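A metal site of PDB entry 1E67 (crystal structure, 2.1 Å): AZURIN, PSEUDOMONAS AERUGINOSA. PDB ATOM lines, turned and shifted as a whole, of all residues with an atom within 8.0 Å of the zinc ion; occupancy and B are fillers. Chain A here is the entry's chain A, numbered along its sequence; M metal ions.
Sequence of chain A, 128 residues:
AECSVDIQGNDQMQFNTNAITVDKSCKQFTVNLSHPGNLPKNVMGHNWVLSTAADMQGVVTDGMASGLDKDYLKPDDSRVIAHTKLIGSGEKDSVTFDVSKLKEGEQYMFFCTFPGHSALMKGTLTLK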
ATOM      1  N   GLY A   9      18.007 -19.104 -21.373  1.00  0.00           N
ATOM      2  CA  GLY A   9      19.275 -18.551 -20.960  1.00  0.00           C
ATOM      3  C   GLY A   9      20.037 -19.706 -20.325  1.00  0.00           C
ATOM      4  O   GLY A   9      19.540 -20.290 -19.347  1.00  0.00           O
ATOM      5  N   ASN A  10      21.196 -20.148 -20.812  1.00  0.00           N
ATOM      6  CA  ASN A  10      21.842 -21.360 -20.287  1.00  0.00           C
ATOM      7  C   ASN A  10      23.099 -21.057 -19.471  1.00  0.00           C
ATOM      8  O   ASN A  10      23.460 -19.893 -19.260  1.00  0.00           O
ATOM      9  CB  ASN A  10      22.197 -22.322 -21.456  1.00  0.00           C
ATOM     10  CG  ASN A  10      23.232 -21.774 -22.430  1.00  0.00           C
ATOM     11  OD1 ASN A  10      24.041 -20.926 -22.068  1.00  0.00           O
ATOM     12  ND2 ASN A  10      23.317 -22.184 -23.683  1.00  0.00           N
ATOM     13  N   MET A  13      26.138 -18.589 -20.697  1.00  0.00           N
ATOM     14  CA  MET A  13      25.802 -17.183 -20.972  1.00  0.00           C
ATOM     15  C   MET A  13      25.342 -16.985 -22.389  1.00  0.00           C
ATOM     16  O   MET A  13      25.831 -16.107 -23.117  1.00  0.00           O
ATOM     17  CB  MET A  13      26.987 -16.196 -20.761  1.00  0.00           C
ATOM     18  CG  MET A  13      27.690 -16.301 -19.427  1.00  0.00           C
ATOM     19  SD  MET A  13      28.814 -14.920 -19.142  1.00  0.00           S
ATOM     20  CE  MET A  13      29.855 -15.189 -20.546  1.00  0.00           C
ATOM     21  N   GLN A  14      24.386 -17.792 -22.812  1.00  0.00           N
ATOM     22  CA  GLN A  14      23.821 -17.695 -24.156  1.00  0.00           C
ATOM     23  C   GLN A  14      22.305 -17.742 -24.128  1.00  0.00           C
ATOM     24  O   GLN A  14      21.712 -18.497 -23.353  1.00  0.00           O
ATOM     25  CB  GLN A  14      24.293 -18.863 -25.031  1.00  0.00           C
ATOM     26  CG  GLN A  14      25.784 -19.001 -25.307  1.00  0.00           C
ATOM     27  CD  GLN A  14      26.167 -20.359 -25.874  1.00  0.00           C
ATOM     28  OE1 GLN A  14      25.624 -21.436 -25.542  1.00  0.00           O
ATOM     29  NE2 GLN A  14      27.153 -20.370 -26.747  1.00  0.00           N
ATOM     30  N   PHE A  15      21.644 -16.942 -24.962  1.00  0.00           N
ATOM     31  CA  PHE A  15      20.197 -16.977 -25.118  1.00  0.00           C
ATOM     32  C   PHE A  15      20.004 -17.840 -26.347  1.00  0.00           C
ATOM     33  O   PHE A  15      20.903 -17.868 -27.200  1.00  0.00           O
ATOM     34  CB  PHE A  15      19.560 -15.635 -25.482  1.00  0.00           C
ATOM     35  CG  PHE A  15      19.403 -14.609 -24.365  1.00  0.00           C
ATOM     36  CD1 PHE A  15      18.709 -14.930 -23.222  1.00  0.00           C
ATOM     37  CD2 PHE A  15      19.889 -13.324 -24.549  1.00  0.00           C
ATOM     38  CE1 PHE A  15      18.503 -13.966 -22.249  1.00  0.00           C
ATOM     39  CE2 PHE A  15      19.669 -12.379 -23.581  1.00  0.00           C
ATOM     40  CZ  PHE A  15      18.981 -12.697 -22.446  1.00  0.00           C
ATOM     41  N   HIS A  35      15.734 -20.942 -17.607  1.00  0.00           N
ATOM     42  CA  HIS A  35      17.160 -21.129 -17.516  1.00  0.00           C
ATOM     43  C   HIS A  35      17.467 -22.610 -17.337  1.00  0.00           C
ATOM     44  O   HIS A  35      17.552 -23.147 -16.218  1.00  0.00           O
ATOM     45  CB  HIS A  35      17.607 -20.285 -16.375  1.00  0.00           C
ATOM     46  CG  HIS A  35      19.087 -20.257 -16.080  1.00  0.00           C
ATOM     47  ND1 HIS A  35      20.028 -21.141 -16.351  1.00  0.00           N
ATOM     48  CD2 HIS A  35      19.660 -19.233 -15.371  1.00  0.00           C
ATOM     49  CE1 HIS A  35      21.151 -20.702 -15.832  1.00  0.00           C
ATOM     50  NE2 HIS A  35      20.929 -19.563 -15.238  1.00  0.00           N
ATOM     51  N   LYS A  41      21.590 -18.349  -9.383  1.00  0.00           N
ATOM     52  CA  LYS A  41      21.377 -16.948  -9.717  1.00  0.00           C
ATOM     53  C   LYS A  41      22.613 -16.094  -9.478  1.00  0.00           C
ATOM     54  O   LYS A  41      22.983 -15.378 -10.407  1.00  0.00           O
ATOM     55  CB  LYS A  41      20.253 -16.446  -8.886  1.00  0.00           C
ATOM     56  CG  LYS A  41      19.675 -15.169  -9.410  1.00  0.00           C
ATOM     57  CD  LYS A  41      19.098 -14.413  -8.234  1.00  0.00           C
ATOM     58  CE  LYS A  41      17.961 -15.146  -7.540  1.00  0.00           C
ATOM     59  NZ  LYS A  41      17.257 -14.225  -6.657  1.00  0.00           N
ATOM     60  N   VAL A  43      25.705 -16.686  -9.728  1.00  0.00           N
ATOM     61  CA  VAL A  43      26.864 -17.026 -10.550  1.00  0.00           C
ATOM     62  C   VAL A  43      26.526 -16.858 -12.025  1.00  0.00           C
ATOM     63  O   VAL A  43      27.349 -16.418 -12.847  1.00  0.00           O
ATOM     64  CB  VAL A  43      27.304 -18.509 -10.289  1.00  0.00           C
ATOM     65  CG1 VAL A  43      28.572 -18.796 -11.021  1.00  0.00           C
ATOM     66  CG2 VAL A  43      27.571 -18.767  -8.842  1.00  0.00           C
ATOM     67  N   MET A  44      25.312 -17.274 -12.374  1.00  0.00           N
ATOM     68  CA  MET A  44      24.863 -17.304 -13.745  1.00  0.00           C
ATOM     69  C   MET A  44      23.457 -16.731 -13.838  1.00  0.00           C
ATOM     70  O   MET A  44      22.631 -17.228 -14.604  1.00  0.00           O
ATOM     71  CB  MET A  44      24.930 -18.765 -14.180  1.00  0.00           C
ATOM     72  CG  MET A  44      24.865 -19.074 -15.679  1.00  0.00           C
ATOM     73  SD  MET A  44      25.961 -18.144 -16.800  1.00  0.00           S
ATOM     74  CE  MET A  44      27.582 -18.448 -16.161  1.00  0.00           C
ATOM     75  N   GLY A  45      23.069 -15.672 -13.137  1.00  0.00           N
ATOM     76  CA  GLY A  45      21.712 -15.102 -13.262  1.00  0.00           C
ATOM     77  C   GLY A  45      21.376 -14.559 -14.653  1.00  0.00           C
ATOM     78  O   GLY A  45      22.268 -14.068 -15.375  1.00  0.00           O
ATOM     79  N   HIS A  46      20.125 -14.680 -15.077  1.00  0.00           N
ATOM     80  CA  HIS A  46      19.735 -14.102 -16.358  1.00  0.00           C
ATOM     81  C   HIS A  46      18.373 -13.484 -16.200  1.00  0.00           C
ATOM     82  O   HIS A  46      17.561 -14.021 -15.456  1.00  0.00           O
ATOM     83  CB  HIS A  46      19.624 -15.140 -17.491  1.00  0.00           C
ATOM     84  CG  HIS A  46      20.863 -15.970 -17.784  1.00  0.00           C
ATOM     85  ND1 HIS A  46      22.084 -15.459 -17.835  1.00  0.00           N
ATOM     86  CD2 HIS A  46      20.854 -17.318 -18.010  1.00  0.00           C
ATOM     87  CE1 HIS A  46      22.852 -16.507 -18.096  1.00  0.00           C
ATOM     88  NE2 HIS A  46      22.115 -17.599 -18.203  1.00  0.00           N
ATOM     89  N   ASN A  47      18.214 -12.314 -16.774  1.00  0.00           N
ATOM     90  CA  ASN A  47      16.918 -11.732 -16.875  1.00  0.00           C
ATOM     91  C   ASN A  47      16.768 -11.367 -18.333  1.00  0.00           C
ATOM     92  O   ASN A  47      17.701 -11.588 -19.106  1.00  0.00           O
ATOM     93  CB  ASN A  47      16.812 -10.518 -15.950  1.00  0.00           C
ATOM     94  CG  ASN A  47      17.927  -9.520 -15.997  1.00  0.00           C
ATOM     95  OD1 ASN A  47      18.702  -9.506 -16.933  1.00  0.00           O
ATOM     96  ND2 ASN A  47      18.121  -8.700 -14.957  1.00  0.00           N
ATOM     97  N   TRP A  48      15.596 -10.970 -18.802  1.00  0.00           N
ATOM     98  CA  TRP A  48      15.367 -10.515 -20.156  1.00  0.00           C
ATOM     99  C   TRP A  48      14.934  -9.061 -19.964  1.00  0.00           C
ATOM    100  O   TRP A  48      13.895  -8.796 -19.340  1.00  0.00           O
ATOM    101  CB  TRP A  48      14.234 -11.330 -20.857  1.00  0.00           C
ATOM    102  CG  TRP A  48      13.958 -10.949 -22.306  1.00  0.00           C
ATOM    103  CD1 TRP A  48      14.664 -11.525 -23.317  1.00  0.00           C
ATOM    104  CD2 TRP A  48      13.050 -10.004 -22.763  1.00  0.00           C
ATOM    105  NE1 TRP A  48      14.206 -10.959 -24.416  1.00  0.00           N
ATOM    106  CE2 TRP A  48      13.244 -10.053 -24.123  1.00  0.00           C
ATOM    107  CE3 TRP A  48      12.107  -9.127 -22.258  1.00  0.00           C
ATOM    108  CZ2 TRP A  48      12.540  -9.255 -24.989  1.00  0.00           C
ATOM    109  CZ3 TRP A  48      11.402  -8.329 -23.138  1.00  0.00           C
ATOM    110  CH2 TRP A  48      11.609  -8.382 -24.493  1.00  0.00           C
ATOM    111  N   LEU A  86      15.477 -11.772 -12.195  1.00  0.00           N
ATOM    112  CA  LEU A  86      16.726 -12.432 -12.506  1.00  0.00           C
ATOM    113  C   LEU A  86      16.486 -13.821 -11.956  1.00  0.00           C
ATOM    114  O   LEU A  86      16.020 -13.945 -10.820  1.00  0.00           O
ATOM    115  CB  LEU A  86      17.887 -11.752 -11.769  1.00  0.00           C
ATOM    116  CG  LEU A  86      19.345 -12.134 -12.038  1.00  0.00           C
ATOM    117  CD1 LEU A  86      19.865 -11.540 -13.351  1.00  0.00           C
ATOM    118  CD2 LEU A  86      20.174 -11.550 -10.899  1.00  0.00           C
ATOM    119  N   ILE A  87      16.734 -14.846 -12.782  1.00  0.00           N
ATOM    120  CA  ILE A  87      16.510 -16.221 -12.410  1.00  0.00           C
ATOM    121  C   ILE A  87      17.764 -17.079 -12.640  1.00  0.00           C
ATOM    122  O   ILE A  87      18.610 -16.847 -13.515  1.00  0.00           O
ATOM    123  CB  ILE A  87      15.306 -16.854 -13.223  1.00  0.00           C
ATOM    124  CG1 ILE A  87      15.577 -16.829 -14.718  1.00  0.00           C
ATOM    125  CG2 ILE A  87      14.019 -16.089 -12.889  1.00  0.00           C
ATOM    126  CD1 ILE A  87      14.576 -17.680 -15.499  1.00  0.00           C
ATOM    127  N   PHE A 111      18.526  -7.901 -23.472  1.00  0.00           N
ATOM    128  CA  PHE A 111      19.822  -8.259 -22.935  1.00  0.00           C
ATOM    129  C   PHE A 111      19.634  -8.701 -21.508  1.00  0.00           C
ATOM    130  O   PHE A 111      18.558  -8.504 -20.929  1.00  0.00           O
ATOM    131  CB  PHE A 111      20.807  -7.061 -22.969  1.00  0.00           C
ATOM    132  CG  PHE A 111      20.195  -5.723 -22.499  1.00  0.00           C
ATOM    133  CD1 PHE A 111      19.487  -4.926 -23.407  1.00  0.00           C
ATOM    134  CD2 PHE A 111      20.348  -5.286 -21.193  1.00  0.00           C
ATOM    135  CE1 PHE A 111      18.935  -3.725 -23.023  1.00  0.00           C
ATOM    136  CE2 PHE A 111      19.794  -4.085 -20.823  1.00  0.00           C
ATOM    137  CZ  PHE A 111      19.092  -3.309 -21.724  1.00  0.00           C
ATOM    138  N   CYS A 112      20.645  -9.351 -20.958  1.00  0.00           N
ATOM    139  CA  CYS A 112      20.694  -9.764 -19.556  1.00  0.00           C
ATOM    140  C   CYS A 112      21.505  -8.665 -18.838  1.00  0.00           C
ATOM    141  O   CYS A 112      22.583  -8.312 -19.357  1.00  0.00           O
ATOM    142  CB  CYS A 112      21.422 -11.093 -19.397  1.00  0.00           C
ATOM    143  SG  CYS A 112      21.574 -11.614 -17.667  1.00  0.00           S
ATOM    144  N   THR A 113      21.110  -8.101 -17.686  1.00  0.00           N
ATOM    145  CA  THR A 113      21.921  -7.083 -17.058  1.00  0.00           C
ATOM    146  C   THR A 113      22.856  -7.637 -16.030  1.00  0.00           C
ATOM    147  O   THR A 113      23.578  -6.862 -15.369  1.00  0.00           O
ATOM    148  CB  THR A 113      21.046  -5.980 -16.386  1.00  0.00           C
ATOM    149  OG1 THR A 113      20.083  -6.611 -15.557  1.00  0.00           O
ATOM    150  CG2 THR A 113      20.348  -5.105 -17.410  1.00  0.00           C
ATOM    151  N   PHE A 114      22.872  -8.968 -15.847  1.00  0.00           N
ATOM    152  CA  PHE A 114      23.763  -9.561 -14.829  1.00  0.00           C
ATOM    153  C   PHE A 114      25.206  -9.212 -15.190  1.00  0.00           C
ATOM    154  O   PHE A 114      25.537  -9.322 -16.375  1.00  0.00           O
ATOM    155  CB  PHE A 114      23.611 -11.120 -14.742  1.00  0.00           C
ATOM    156  CG  PHE A 114      24.446 -11.797 -13.633  1.00  0.00           C
ATOM    157  CD1 PHE A 114      25.752 -12.213 -13.869  1.00  0.00           C
ATOM    158  CD2 PHE A 114      23.904 -12.040 -12.382  1.00  0.00           C
ATOM    159  CE1 PHE A 114      26.499 -12.847 -12.882  1.00  0.00           C
ATOM    160  CE2 PHE A 114      24.645 -12.677 -11.402  1.00  0.00           C
ATOM    161  CZ  PHE A 114      25.940 -13.077 -11.651  1.00  0.00           C
ATOM    162  N   PRO A 115      26.084  -8.816 -14.249  1.00  0.00           N
ATOM    163  CA  PRO A 115      27.408  -8.329 -14.527  1.00  0.00           C
ATOM    164  C   PRO A 115      28.201  -9.181 -15.524  1.00  0.00           C
ATOM    165  O   PRO A 115      28.348 -10.385 -15.318  1.00  0.00           O
ATOM    166  CB  PRO A 115      28.044  -8.266 -13.163  1.00  0.00           C
ATOM    167  CG  PRO A 115      26.910  -7.995 -12.249  1.00  0.00           C
ATOM    168  CD  PRO A 115      25.857  -8.894 -12.812  1.00  0.00           C
ATOM    169  N   GLY A 116      28.587  -8.614 -16.657  1.00  0.00           N
ATOM    170  CA  GLY A 116      29.410  -9.320 -17.617  1.00  0.00           C
ATOM    171  C   GLY A 116      28.631 -10.098 -18.678  1.00  0.00           C
ATOM    172  O   GLY A 116      29.201 -10.405 -19.741  1.00  0.00           O
ATOM    173  N   HIS A 117      27.334 -10.379 -18.456  1.00  0.00           N
ATOM    174  CA  HIS A 117      26.581 -11.132 -19.420  1.00  0.00           C
ATOM    175  C   HIS A 117      26.118 -10.331 -20.637  1.00  0.00           C
ATOM    176  O   HIS A 117      26.121 -10.925 -21.731  1.00  0.00           O
ATOM    177  CB  HIS A 117      25.360 -11.751 -18.785  1.00  0.00           C
ATOM    178  CG  HIS A 117      25.678 -12.847 -17.771  1.00  0.00           C
ATOM    179  ND1 HIS A 117      24.736 -13.665 -17.344  1.00  0.00           N
ATOM    180  CD2 HIS A 117      26.905 -13.152 -17.273  1.00  0.00           C
ATOM    181  CE1 HIS A 117      25.378 -14.522 -16.565  1.00  0.00           C
ATOM    182  NE2 HIS A 117      26.649 -14.205 -16.537  1.00  0.00           N
ATOM    183  N   SER A 118      25.752  -9.045 -20.581  1.00  0.00           N
ATOM    184  CA  SER A 118      25.204  -8.356 -21.754  1.00  0.00           C
ATOM    185  C   SER A 118      26.097  -8.332 -22.983  1.00  0.00           C
ATOM    186  O   SER A 118      25.596  -8.296 -24.096  1.00  0.00           O
ATOM    187  CB  SER A 118      24.830  -6.905 -21.388  1.00  0.00           C
ATOM    188  OG  SER A 118      25.933  -6.101 -21.004  1.00  0.00           O
ATOM    189  N   MET A 121      25.000 -11.718 -24.064  1.00  0.00           N
ATOM    190  CA  MET A 121      23.593 -12.015 -23.983  1.00  0.00           C
ATOM    191  C   MET A 121      22.784 -10.811 -24.432  1.00  0.00           C
ATOM    192  O   MET A 121      22.401  -9.963 -23.627  1.00  0.00           O
ATOM    193  CB  MET A 121      23.223 -12.392 -22.565  1.00  0.00           C
ATOM    194  CG  MET A 121      23.981 -13.650 -22.126  1.00  0.00           C
ATOM    195  SD  MET A 121      23.370 -14.422 -20.618  1.00  0.00           S
ATOM    196  CE  MET A 121      21.991 -15.341 -21.256  1.00  0.00           C
HETATM  197 ZN    ZN M   1      22.690 -13.586 -17.472  1.00  0.00          ZN
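The backbone NH (N) of Phe 114 lies close to the side-chain sulfur (SG) of Cys 112 (3.5 Å). The backbone NH (N) of Cys 112 sits at hydrogen-bond distance from the backbone carbonyl oxygen (O) of Met 121, 3.3 Å away. O of Cys 112 lies close to N of Ser 118. ND1 of His 117 lies close to SD of Met 121. A ring nitrogen (ND1) of His 46 sits close to the side-chain sulfur (SD) of Met 121 (3.2 Å). A ring nitrogen (NE2) of His 46 sits at hydrogen-bond distance from the backbone carbonyl oxygen of Asn 10. The side-chain sulfur (SD) of Met 13 sits close to a ring nitrogen (NE2) of His 117, 3.5 Å away. O of His 46 is in hydrogen-bond range of N of Ile 87 (2.9 Å).
Merely in contact with the zinc ion: Met 121 (3.3 Å) and Phe 114 (3.8 Å). Of the 24 residues printed, 6 come within 4 Å of the zinc ion. The nearest printed residue that does not touch the zinc ion is Met 44 (4.6 Å).
The zinc ion is bound by ND1 of His 46 (2.0 Å), ND1 of His 117 (2.1 Å), O of Gly 45 (2.2 Å) and SG of Cys 112 (2.3 Å). The zinc ion has four donor atoms within binding distance.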
